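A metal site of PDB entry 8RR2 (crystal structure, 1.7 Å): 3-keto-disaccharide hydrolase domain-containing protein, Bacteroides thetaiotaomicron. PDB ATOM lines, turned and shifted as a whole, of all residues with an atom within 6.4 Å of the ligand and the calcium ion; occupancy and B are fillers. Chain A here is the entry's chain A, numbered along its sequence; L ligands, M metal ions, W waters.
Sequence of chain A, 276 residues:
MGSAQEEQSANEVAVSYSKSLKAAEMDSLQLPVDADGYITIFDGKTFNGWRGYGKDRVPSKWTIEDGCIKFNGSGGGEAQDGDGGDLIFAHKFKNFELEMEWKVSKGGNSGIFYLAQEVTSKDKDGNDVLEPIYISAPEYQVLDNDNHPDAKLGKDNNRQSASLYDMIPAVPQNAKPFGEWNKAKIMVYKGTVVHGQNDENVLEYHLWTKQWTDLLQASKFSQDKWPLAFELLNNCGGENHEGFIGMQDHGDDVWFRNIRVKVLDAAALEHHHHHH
OE2 of Glu 78 is in hydrogen-bond range of O6 of the ligand (2.5 Å). A ring nitrogen (NE2) of His 250 is in hydrogen-bond range of an oxygen (O6) of the ligand, 2.7 Å away. OD2 of Asp 150 is in hydrogen-bond range of O2 of the ligand (2.7 Å). An oxygen (O4) of the ligand is in hydrogen-bond range of the side-chain amino group (NZ) of Lys 220 (2.9 Å).
The side-chain amide nitrogen (NE2) of Gln 141 sits at hydrogen-bond distance from the backbone carbonyl oxygen (O) of Arg 159 (2.9 Å). The backbone carbonyl oxygen of Val 142 is in hydrogen-bond range of the backbone NH of Ser 110 (2.8 Å). The backbone NH (N) of Gln 248 is in hydrogen-bond range of the backbone carbonyl oxygen (O) of Gly 111. N of Asp 150 lies within hydrogen-bond range of ND1 of His 148 (3.1 Å). The side-chain amide nitrogen of Asn 109 is in hydrogen-bond range of the side-chain carboxylate of Asp 150 (2.9 Å). The side-chain hydroxyl (OH) of Tyr 165 lies close to the guanidinium group (NE) of Arg 159. The backbone NH (N) of Lys 220 lies within hydrogen-bond range of the side-chain carboxylate (OD2) of Asp 166 (2.9 Å). The backbone carbonyl oxygen (O) of Glu 139 is in hydrogen-bond range of the backbone NH (N) of Tyr 165, at 3.1 Å.
Tyr 134 touches the ligand. Tyr 165 touches the ligand (OH to C6, 3.2 Å). Phe 221 touches the ligand. Of the 21 residues printed, 11 come within 4 Å of the ligand.
Along chain A the residues within 4 Å of the calcium ion span positions 109 to 248.
OE1 of Gln 141 is bound to the calcium ion (2.3 Å). The side-chain carboxylate (OE2) of Glu 139 is bound to the calcium ion (2.4 Å). The calcium ion is bound by the side-chain amide oxygen (OE1) of Gln 248. The backbone carbonyl oxygen (O) of Ser 110 binds the calcium ion (2.5 Å). The calcium ion is bound by O3 of the ligand (2.5 Å). OD1 of Asn 109 is bound to the calcium ion, at 2.5 Å. The calcium ion is bound by O1 of the ligand. The calcium ion has seven donor atoms within binding distance.
Water W2 lies within hydrogen-bond range of O2 of the ligand and OD1 of Asp 150. Water W1 bridges the side-chain carboxylate of Glu 139 and an oxygen (O4) of the ligand.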
ATOM      1  N   GLY A  77      -5.018 -28.763 -16.380  1.00  0.00           N
ATOM      2  CA  GLY A  77      -4.011 -27.857 -15.849  1.00  0.00           C
ATOM      3  C   GLY A  77      -2.593 -28.260 -16.213  1.00  0.00           C
ATOM      4  O   GLY A  77      -2.237 -28.419 -17.389  1.00  0.00           O
ATOM      5  N   GLU A  78      -1.758 -28.420 -15.200  1.00  0.00           N
ATOM      6  CA  GLU A  78      -0.354 -28.820 -15.421  1.00  0.00           C
ATOM      7  C   GLU A  78      -0.201 -30.280 -15.807  1.00  0.00           C
ATOM      8  O   GLU A  78       0.933 -30.717 -16.046  1.00  0.00           O
ATOM      9  CB  GLU A  78       0.471 -28.571 -14.157  1.00  0.00           C
ATOM     10  CG  GLU A  78       0.780 -27.104 -13.855  1.00  0.00           C
ATOM     11  CD  GLU A  78       1.780 -26.973 -12.702  1.00  0.00           C
ATOM     12  OE1 GLU A  78       2.331 -28.020 -12.245  1.00  0.00           O
ATOM     13  OE2 GLU A  78       1.971 -25.838 -12.234  1.00  0.00           O
ATOM     14  N   ASN A 109      -5.951 -20.776 -19.532  1.00  0.00           N
ATOM     15  CA  ASN A 109      -4.575 -20.453 -19.139  1.00  0.00           C
ATOM     16  C   ASN A 109      -3.664 -21.073 -20.183  1.00  0.00           C
ATOM     17  O   ASN A 109      -3.852 -22.234 -20.546  1.00  0.00           O
ATOM     18  CB  ASN A 109      -4.279 -21.003 -17.714  1.00  0.00           C
ATOM     19  CG  ASN A 109      -2.810 -20.810 -17.234  1.00  0.00           C
ATOM     20  OD1 ASN A 109      -1.852 -20.820 -17.991  1.00  0.00           O
ATOM     21  ND2 ASN A 109      -2.660 -20.619 -15.923  1.00  0.00           N
ATOM     22  N   SER A 110      -2.667 -20.308 -20.645  1.00  0.00           N
ATOM     23  CA  SER A 110      -1.563 -20.849 -21.449  1.00  0.00           C
ATOM     24  C   SER A 110      -0.375 -19.922 -21.198  1.00  0.00           C
ATOM     25  O   SER A 110      -0.284 -19.339 -20.119  1.00  0.00           O
ATOM     26  CB  SER A 110      -1.936 -20.907 -22.936  1.00  0.00           C
ATOM     27  OG  SER A 110      -0.910 -21.488 -23.728  1.00  0.00           O
ATOM     28  N   GLY A 111       0.527 -19.788 -22.134  1.00  0.00           N
ATOM     29  CA  GLY A 111       1.668 -18.903 -21.923  1.00  0.00           C
ATOM     30  C   GLY A 111       2.527 -18.914 -23.167  1.00  0.00           C
ATOM     31  O   GLY A 111       2.460 -19.831 -23.983  1.00  0.00           O
ATOM     32  N   PHE A 113       6.460 -18.844 -24.095  1.00  0.00           N
ATOM     33  CA  PHE A 113       7.785 -18.997 -23.522  1.00  0.00           C
ATOM     34  C   PHE A 113       8.837 -18.423 -24.442  1.00  0.00           C
ATOM     35  O   PHE A 113       8.647 -18.370 -25.665  1.00  0.00           O
ATOM     36  CB  PHE A 113       8.132 -20.476 -23.276  1.00  0.00           C
ATOM     37  CG  PHE A 113       7.213 -21.156 -22.308  1.00  0.00           C
ATOM     38  CD1 PHE A 113       7.280 -20.851 -20.951  1.00  0.00           C
ATOM     39  CD2 PHE A 113       6.290 -22.099 -22.738  1.00  0.00           C
ATOM     40  CE1 PHE A 113       6.404 -21.471 -20.037  1.00  0.00           C
ATOM     41  CE2 PHE A 113       5.441 -22.727 -21.839  1.00  0.00           C
ATOM     42  CZ  PHE A 113       5.499 -22.411 -20.484  1.00  0.00           C
ATOM     43  N   TYR A 134       9.243 -24.498 -18.313  1.00  0.00           N
ATOM     44  CA  TYR A 134       9.204 -23.222 -17.607  1.00  0.00           C
ATOM     45  C   TYR A 134      10.236 -23.093 -16.505  1.00  0.00           C
ATOM     46  O   TYR A 134      10.326 -22.007 -15.917  1.00  0.00           O
ATOM     47  CB  TYR A 134       7.803 -22.965 -17.054  1.00  0.00           C
ATOM     48  CG  TYR A 134       7.316 -24.015 -16.097  1.00  0.00           C
ATOM     49  CD1 TYR A 134       7.805 -24.098 -14.797  1.00  0.00           C
ATOM     50  CD2 TYR A 134       6.357 -24.963 -16.495  1.00  0.00           C
ATOM     51  CE1 TYR A 134       7.342 -25.078 -13.903  1.00  0.00           C
ATOM     52  CE2 TYR A 134       5.896 -25.940 -15.592  1.00  0.00           C
ATOM     53  CZ  TYR A 134       6.400 -25.978 -14.311  1.00  0.00           C
ATOM     54  OH  TYR A 134       5.966 -26.964 -13.422  1.00  0.00           O
ATOM     55  N   GLU A 139       8.215 -16.826 -18.849  1.00  0.00           N
ATOM     56  CA  GLU A 139       6.893 -17.029 -19.418  1.00  0.00           C
ATOM     57  C   GLU A 139       6.127 -15.704 -19.474  1.00  0.00           C
ATOM     58  O   GLU A 139       6.008 -15.014 -18.467  1.00  0.00           O
ATOM     59  CB  GLU A 139       6.105 -18.086 -18.579  1.00  0.00           C
ATOM     60  CG  GLU A 139       4.699 -18.214 -19.121  1.00  0.00           C
ATOM     61  CD  GLU A 139       3.802 -19.117 -18.309  1.00  0.00           C
ATOM     62  OE1 GLU A 139       4.259 -19.735 -17.292  1.00  0.00           O
ATOM     63  OE2 GLU A 139       2.612 -19.196 -18.681  1.00  0.00           O
ATOM     64  N   TYR A 140       5.605 -15.384 -20.642  1.00  0.00           N
ATOM     65  CA  TYR A 140       4.601 -14.344 -20.789  1.00  0.00           C
ATOM     66  C   TYR A 140       3.267 -15.044 -20.549  1.00  0.00           C
ATOM     67  O   TYR A 140       2.818 -15.833 -21.380  1.00  0.00           O
ATOM     68  CB  TYR A 140       4.721 -13.751 -22.191  1.00  0.00           C
ATOM     69  CG  TYR A 140       3.713 -12.733 -22.677  1.00  0.00           C
ATOM     70  CD1 TYR A 140       2.378 -13.068 -22.891  1.00  0.00           C
ATOM     71  CD2 TYR A 140       4.129 -11.448 -23.013  1.00  0.00           C
ATOM     72  CE1 TYR A 140       1.462 -12.106 -23.381  1.00  0.00           C
ATOM     73  CE2 TYR A 140       3.222 -10.466 -23.534  1.00  0.00           C
ATOM     74  CZ  TYR A 140       1.890 -10.829 -23.706  1.00  0.00           C
ATOM     75  OH  TYR A 140       1.017  -9.867 -24.185  1.00  0.00           O
ATOM     76  N   GLN A 141       2.656 -14.803 -19.382  1.00  0.00           N
ATOM     77  CA  GLN A 141       1.418 -15.484 -19.031  1.00  0.00           C
ATOM     78  C   GLN A 141       0.326 -15.160 -20.037  1.00  0.00           C
ATOM     79  O   GLN A 141       0.196 -14.023 -20.490  1.00  0.00           O
ATOM     80  CB  GLN A 141       0.960 -15.035 -17.637  1.00  0.00           C
ATOM     81  CG  GLN A 141      -0.399 -15.555 -17.215  1.00  0.00           C
ATOM     82  CD  GLN A 141      -0.374 -16.984 -16.742  1.00  0.00           C
ATOM     83  OE1 GLN A 141       0.050 -17.907 -17.471  1.00  0.00           O
ATOM     84  NE2 GLN A 141      -0.836 -17.202 -15.517  1.00  0.00           N
ATOM     85  N   VAL A 142      -0.468 -16.167 -20.368  1.00  0.00           N
ATOM     86  CA  VAL A 142      -1.683 -16.030 -21.169  1.00  0.00           C
ATOM     87  C   VAL A 142      -2.846 -16.497 -20.291  1.00  0.00           C
ATOM     88  O   VAL A 142      -2.811 -17.613 -19.757  1.00  0.00           O
ATOM     89  CB  VAL A 142      -1.570 -16.851 -22.466  1.00  0.00           C
ATOM     90  CG1 VAL A 142      -2.954 -17.117 -23.138  1.00  0.00           C
ATOM     91  CG2 VAL A 142      -0.597 -16.165 -23.428  1.00  0.00           C
ATOM     92  N   LEU A 143      -3.867 -15.657 -20.146  1.00  0.00           N
ATOM     93  CA  LEU A 143      -4.849 -15.941 -19.095  1.00  0.00           C
ATOM     94  C   LEU A 143      -6.164 -15.219 -19.357  1.00  0.00           C
ATOM     95  O   LEU A 143      -6.191 -14.115 -19.890  1.00  0.00           O
ATOM     96  CB  LEU A 143      -4.311 -15.508 -17.726  1.00  0.00           C
ATOM     97  CG  LEU A 143      -5.084 -16.115 -16.548  1.00  0.00           C
ATOM     98  CD1 LEU A 143      -4.601 -17.565 -16.378  1.00  0.00           C
ATOM     99  CD2 LEU A 143      -4.846 -15.379 -15.276  1.00  0.00           C
ATOM    100  N   HIS A 148      -9.979 -17.123 -14.442  1.00  0.00           N
ATOM    101  CA  HIS A 148      -9.036 -18.116 -13.938  1.00  0.00           C
ATOM    102  C   HIS A 148      -8.487 -17.685 -12.571  1.00  0.00           C
ATOM    103  O   HIS A 148      -8.070 -16.535 -12.414  1.00  0.00           O
ATOM    104  CB  HIS A 148      -7.866 -18.284 -14.899  1.00  0.00           C
ATOM    105  CG  HIS A 148      -7.102 -19.550 -14.690  1.00  0.00           C
ATOM    106  ND1 HIS A 148      -6.302 -19.767 -13.583  1.00  0.00           N
ATOM    107  CD2 HIS A 148      -6.992 -20.665 -15.459  1.00  0.00           C
ATOM    108  CE1 HIS A 148      -5.745 -20.969 -13.671  1.00  0.00           C
ATOM    109  NE2 HIS A 148      -6.162 -21.539 -14.794  1.00  0.00           N
ATOM    110  N   ASP A 150      -5.667 -18.046 -11.123  1.00  0.00           N
ATOM    111  CA  ASP A 150      -4.331 -17.426 -11.150  1.00  0.00           C
ATOM    112  C   ASP A 150      -4.396 -15.914 -11.021  1.00  0.00           C
ATOM    113  O   ASP A 150      -3.471 -15.282 -10.472  1.00  0.00           O
ATOM    114  CB  ASP A 150      -3.570 -17.727 -12.453  1.00  0.00           C
ATOM    115  CG  ASP A 150      -2.824 -19.012 -12.385  1.00  0.00           C
ATOM    116  OD1 ASP A 150      -2.955 -19.691 -11.352  1.00  0.00           O
ATOM    117  OD2 ASP A 150      -2.099 -19.324 -13.359  1.00  0.00           O
ATOM    118  N   ARG A 159       0.439 -12.836 -11.845  1.00  0.00           N
ATOM    119  CA  ARG A 159       0.080 -14.037 -12.597  1.00  0.00           C
ATOM    120  C   ARG A 159      -1.013 -13.762 -13.619  1.00  0.00           C
ATOM    121  O   ARG A 159      -1.570 -14.708 -14.193  1.00  0.00           O
ATOM    122  CB  ARG A 159      -0.326 -15.160 -11.635  1.00  0.00           C
ATOM    123  CG  ARG A 159       0.855 -15.537 -10.709  1.00  0.00           C
ATOM    124  CD  ARG A 159       0.498 -16.729  -9.800  1.00  0.00           C
ATOM    125  NE  ARG A 159       1.600 -17.024  -8.882  1.00  0.00           N
ATOM    126  CZ  ARG A 159       1.578 -18.019  -7.995  1.00  0.00           C
ATOM    127  NH1 ARG A 159       0.541 -18.849  -7.914  1.00  0.00           N
ATOM    128  NH2 ARG A 159       2.623 -18.185  -7.185  1.00  0.00           N
ATOM    129  N   TYR A 165       5.519 -14.390 -15.494  1.00  0.00           N
ATOM    130  CA  TYR A 165       4.802 -15.210 -14.517  1.00  0.00           C
ATOM    131  C   TYR A 165       5.507 -15.297 -13.159  1.00  0.00           C
ATOM    132  O   TYR A 165       6.649 -15.731 -13.074  1.00  0.00           O
ATOM    133  CB  TYR A 165       4.572 -16.637 -15.058  1.00  0.00           C
ATOM    134  CG  TYR A 165       3.752 -17.409 -14.073  1.00  0.00           C
ATOM    135  CD1 TYR A 165       2.363 -17.327 -14.060  1.00  0.00           C
ATOM    136  CD2 TYR A 165       4.382 -18.200 -13.114  1.00  0.00           C
ATOM    137  CE1 TYR A 165       1.629 -18.009 -13.094  1.00  0.00           C
ATOM    138  CE2 TYR A 165       3.655 -18.857 -12.137  1.00  0.00           C
ATOM    139  CZ  TYR A 165       2.283 -18.767 -12.154  1.00  0.00           C
ATOM    140  OH  TYR A 165       1.538 -19.435 -11.212  1.00  0.00           O
ATOM    141  N   ASP A 166       4.801 -14.905 -12.109  1.00  0.00           N
ATOM    142  CA  ASP A 166       5.240 -14.964 -10.706  1.00  0.00           C
ATOM    143  C   ASP A 166       6.352 -14.004 -10.394  1.00  0.00           C
ATOM    144  O   ASP A 166       6.957 -14.131  -9.314  1.00  0.00           O
ATOM    145  CB  ASP A 166       5.659 -16.373 -10.252  1.00  0.00           C
ATOM    146  CG  ASP A 166       5.398 -16.595  -8.770  1.00  0.00           C
ATOM    147  OD1 ASP A 166       4.332 -16.145  -8.281  1.00  0.00           O
ATOM    148  OD2 ASP A 166       6.263 -17.197  -8.089  1.00  0.00           O
ATOM    149  N   LYS A 220       8.628 -18.524  -7.147  1.00  0.00           N
ATOM    150  CA  LYS A 220       8.551 -19.973  -7.045  1.00  0.00           C
ATOM    151  C   LYS A 220       9.823 -20.641  -7.530  1.00  0.00           C
ATOM    152  O   LYS A 220      10.015 -21.854  -7.284  1.00  0.00           O
ATOM    153  CB  LYS A 220       7.373 -20.520  -7.877  1.00  0.00           C
ATOM    154  CG  LYS A 220       7.478 -20.187  -9.369  1.00  0.00           C
ATOM    155  CD  LYS A 220       6.247 -20.616 -10.164  1.00  0.00           C
ATOM    156  CE  LYS A 220       6.117 -22.125 -10.235  1.00  0.00           C
ATOM    157  NZ  LYS A 220       4.893 -22.513 -11.034  1.00  0.00           N
ATOM    158  N   PHE A 221      10.671 -19.915  -8.257  1.00  0.00           N
ATOM    159  CA  PHE A 221      11.902 -20.472  -8.804  1.00  0.00           C
ATOM    160  C   PHE A 221      13.123 -20.071  -7.975  1.00  0.00           C
ATOM    161  O   PHE A 221      14.240 -20.065  -8.495  1.00  0.00           O
ATOM    162  CB  PHE A 221      12.096 -20.037 -10.256  1.00  0.00           C
ATOM    163  CG  PHE A 221      10.928 -20.363 -11.157  1.00  0.00           C
ATOM    164  CD1 PHE A 221      10.541 -21.670 -11.376  1.00  0.00           C
ATOM    165  CD2 PHE A 221      10.244 -19.339 -11.803  1.00  0.00           C
ATOM    166  CE1 PHE A 221       9.450 -21.973 -12.217  1.00  0.00           C
ATOM    167  CE2 PHE A 221       9.176 -19.618 -12.658  1.00  0.00           C
ATOM    168  CZ  PHE A 221       8.791 -20.930 -12.864  1.00  0.00           C
ATOM    169  N   GLN A 248       2.309 -22.827 -24.289  1.00  0.00           N
ATOM    170  CA  GLN A 248       2.094 -23.714 -23.152  1.00  0.00           C
ATOM    171  C   GLN A 248       0.864 -24.607 -23.328  1.00  0.00           C
ATOM    172  O   GLN A 248      -0.234 -24.105 -23.643  1.00  0.00           O
ATOM    173  CB  GLN A 248       1.916 -22.891 -21.872  1.00  0.00           C
ATOM    174  CG  GLN A 248       1.853 -23.812 -20.663  1.00  0.00           C
ATOM    175  CD  GLN A 248       1.751 -23.013 -19.394  1.00  0.00           C
ATOM    176  OE1 GLN A 248       1.019 -22.047 -19.332  1.00  0.00           O
ATOM    177  NE2 GLN A 248       2.555 -23.371 -18.402  1.00  0.00           N
ATOM    178  N   HIS A 250      -1.467 -25.892 -20.936  1.00  0.00           N
ATOM    179  CA  HIS A 250      -1.959 -25.830 -19.551  1.00  0.00           C
ATOM    180  C   HIS A 250      -3.381 -26.369 -19.509  1.00  0.00           C
ATOM    181  O   HIS A 250      -4.195 -25.951 -18.680  1.00  0.00           O
ATOM    182  CB  HIS A 250      -1.871 -24.417 -18.980  1.00  0.00           C
ATOM    183  CG  HIS A 250      -1.764 -24.355 -17.483  1.00  0.00           C
ATOM    184  ND1 HIS A 250      -2.867 -24.256 -16.654  1.00  0.00           N
ATOM    185  CD2 HIS A 250      -0.684 -24.405 -16.667  1.00  0.00           C
ATOM    186  CE1 HIS A 250      -2.460 -24.245 -15.388  1.00  0.00           C
ATOM    187  NE2 HIS A 250      -1.139 -24.329 -15.372  1.00  0.00           N
HETATM  188  C1  LIG L   1       4.453 -22.616 -14.557  1.00  0.00           C
HETATM  189  C2  LIG L   1       1.188 -22.757 -12.834  1.00  0.00           C
HETATM  190  C3  LIG L   1       0.891 -21.168 -14.754  1.00  0.00           C
HETATM  191  C4  LIG L   1       2.377 -21.284 -15.051  1.00  0.00           C
HETATM  192  C5  LIG L   1       2.937 -22.566 -14.469  1.00  0.00           C
HETATM  193  C6  LIG L   1       0.433 -21.533 -13.347  1.00  0.00           C
HETATM  194  O1  LIG L   1       2.556 -21.231 -16.463  1.00  0.00           O
HETATM  195  O2  LIG L   1      -0.966 -21.726 -13.323  1.00  0.00           O
HETATM  196  O3  LIG L   1       0.132 -20.694 -15.569  1.00  0.00           O
HETATM  197  O4  LIG L   1       5.071 -21.607 -13.769  1.00  0.00           O
HETATM  198  O5  LIG L   1       2.595 -22.647 -13.071  1.00  0.00           O
HETATM  199  O6  LIG L   1       0.679 -23.975 -13.369  1.00  0.00           O
HETATM  200 CA    CA M   1       0.562 -20.140 -17.959  1.00  0.00          CA
HETATM  201  O   HOH W   1       6.262 -19.853 -15.475  1.00  0.00           O
HETATM  202  O   HOH W   2      -2.841 -22.586 -11.673  1.00  0.00           O
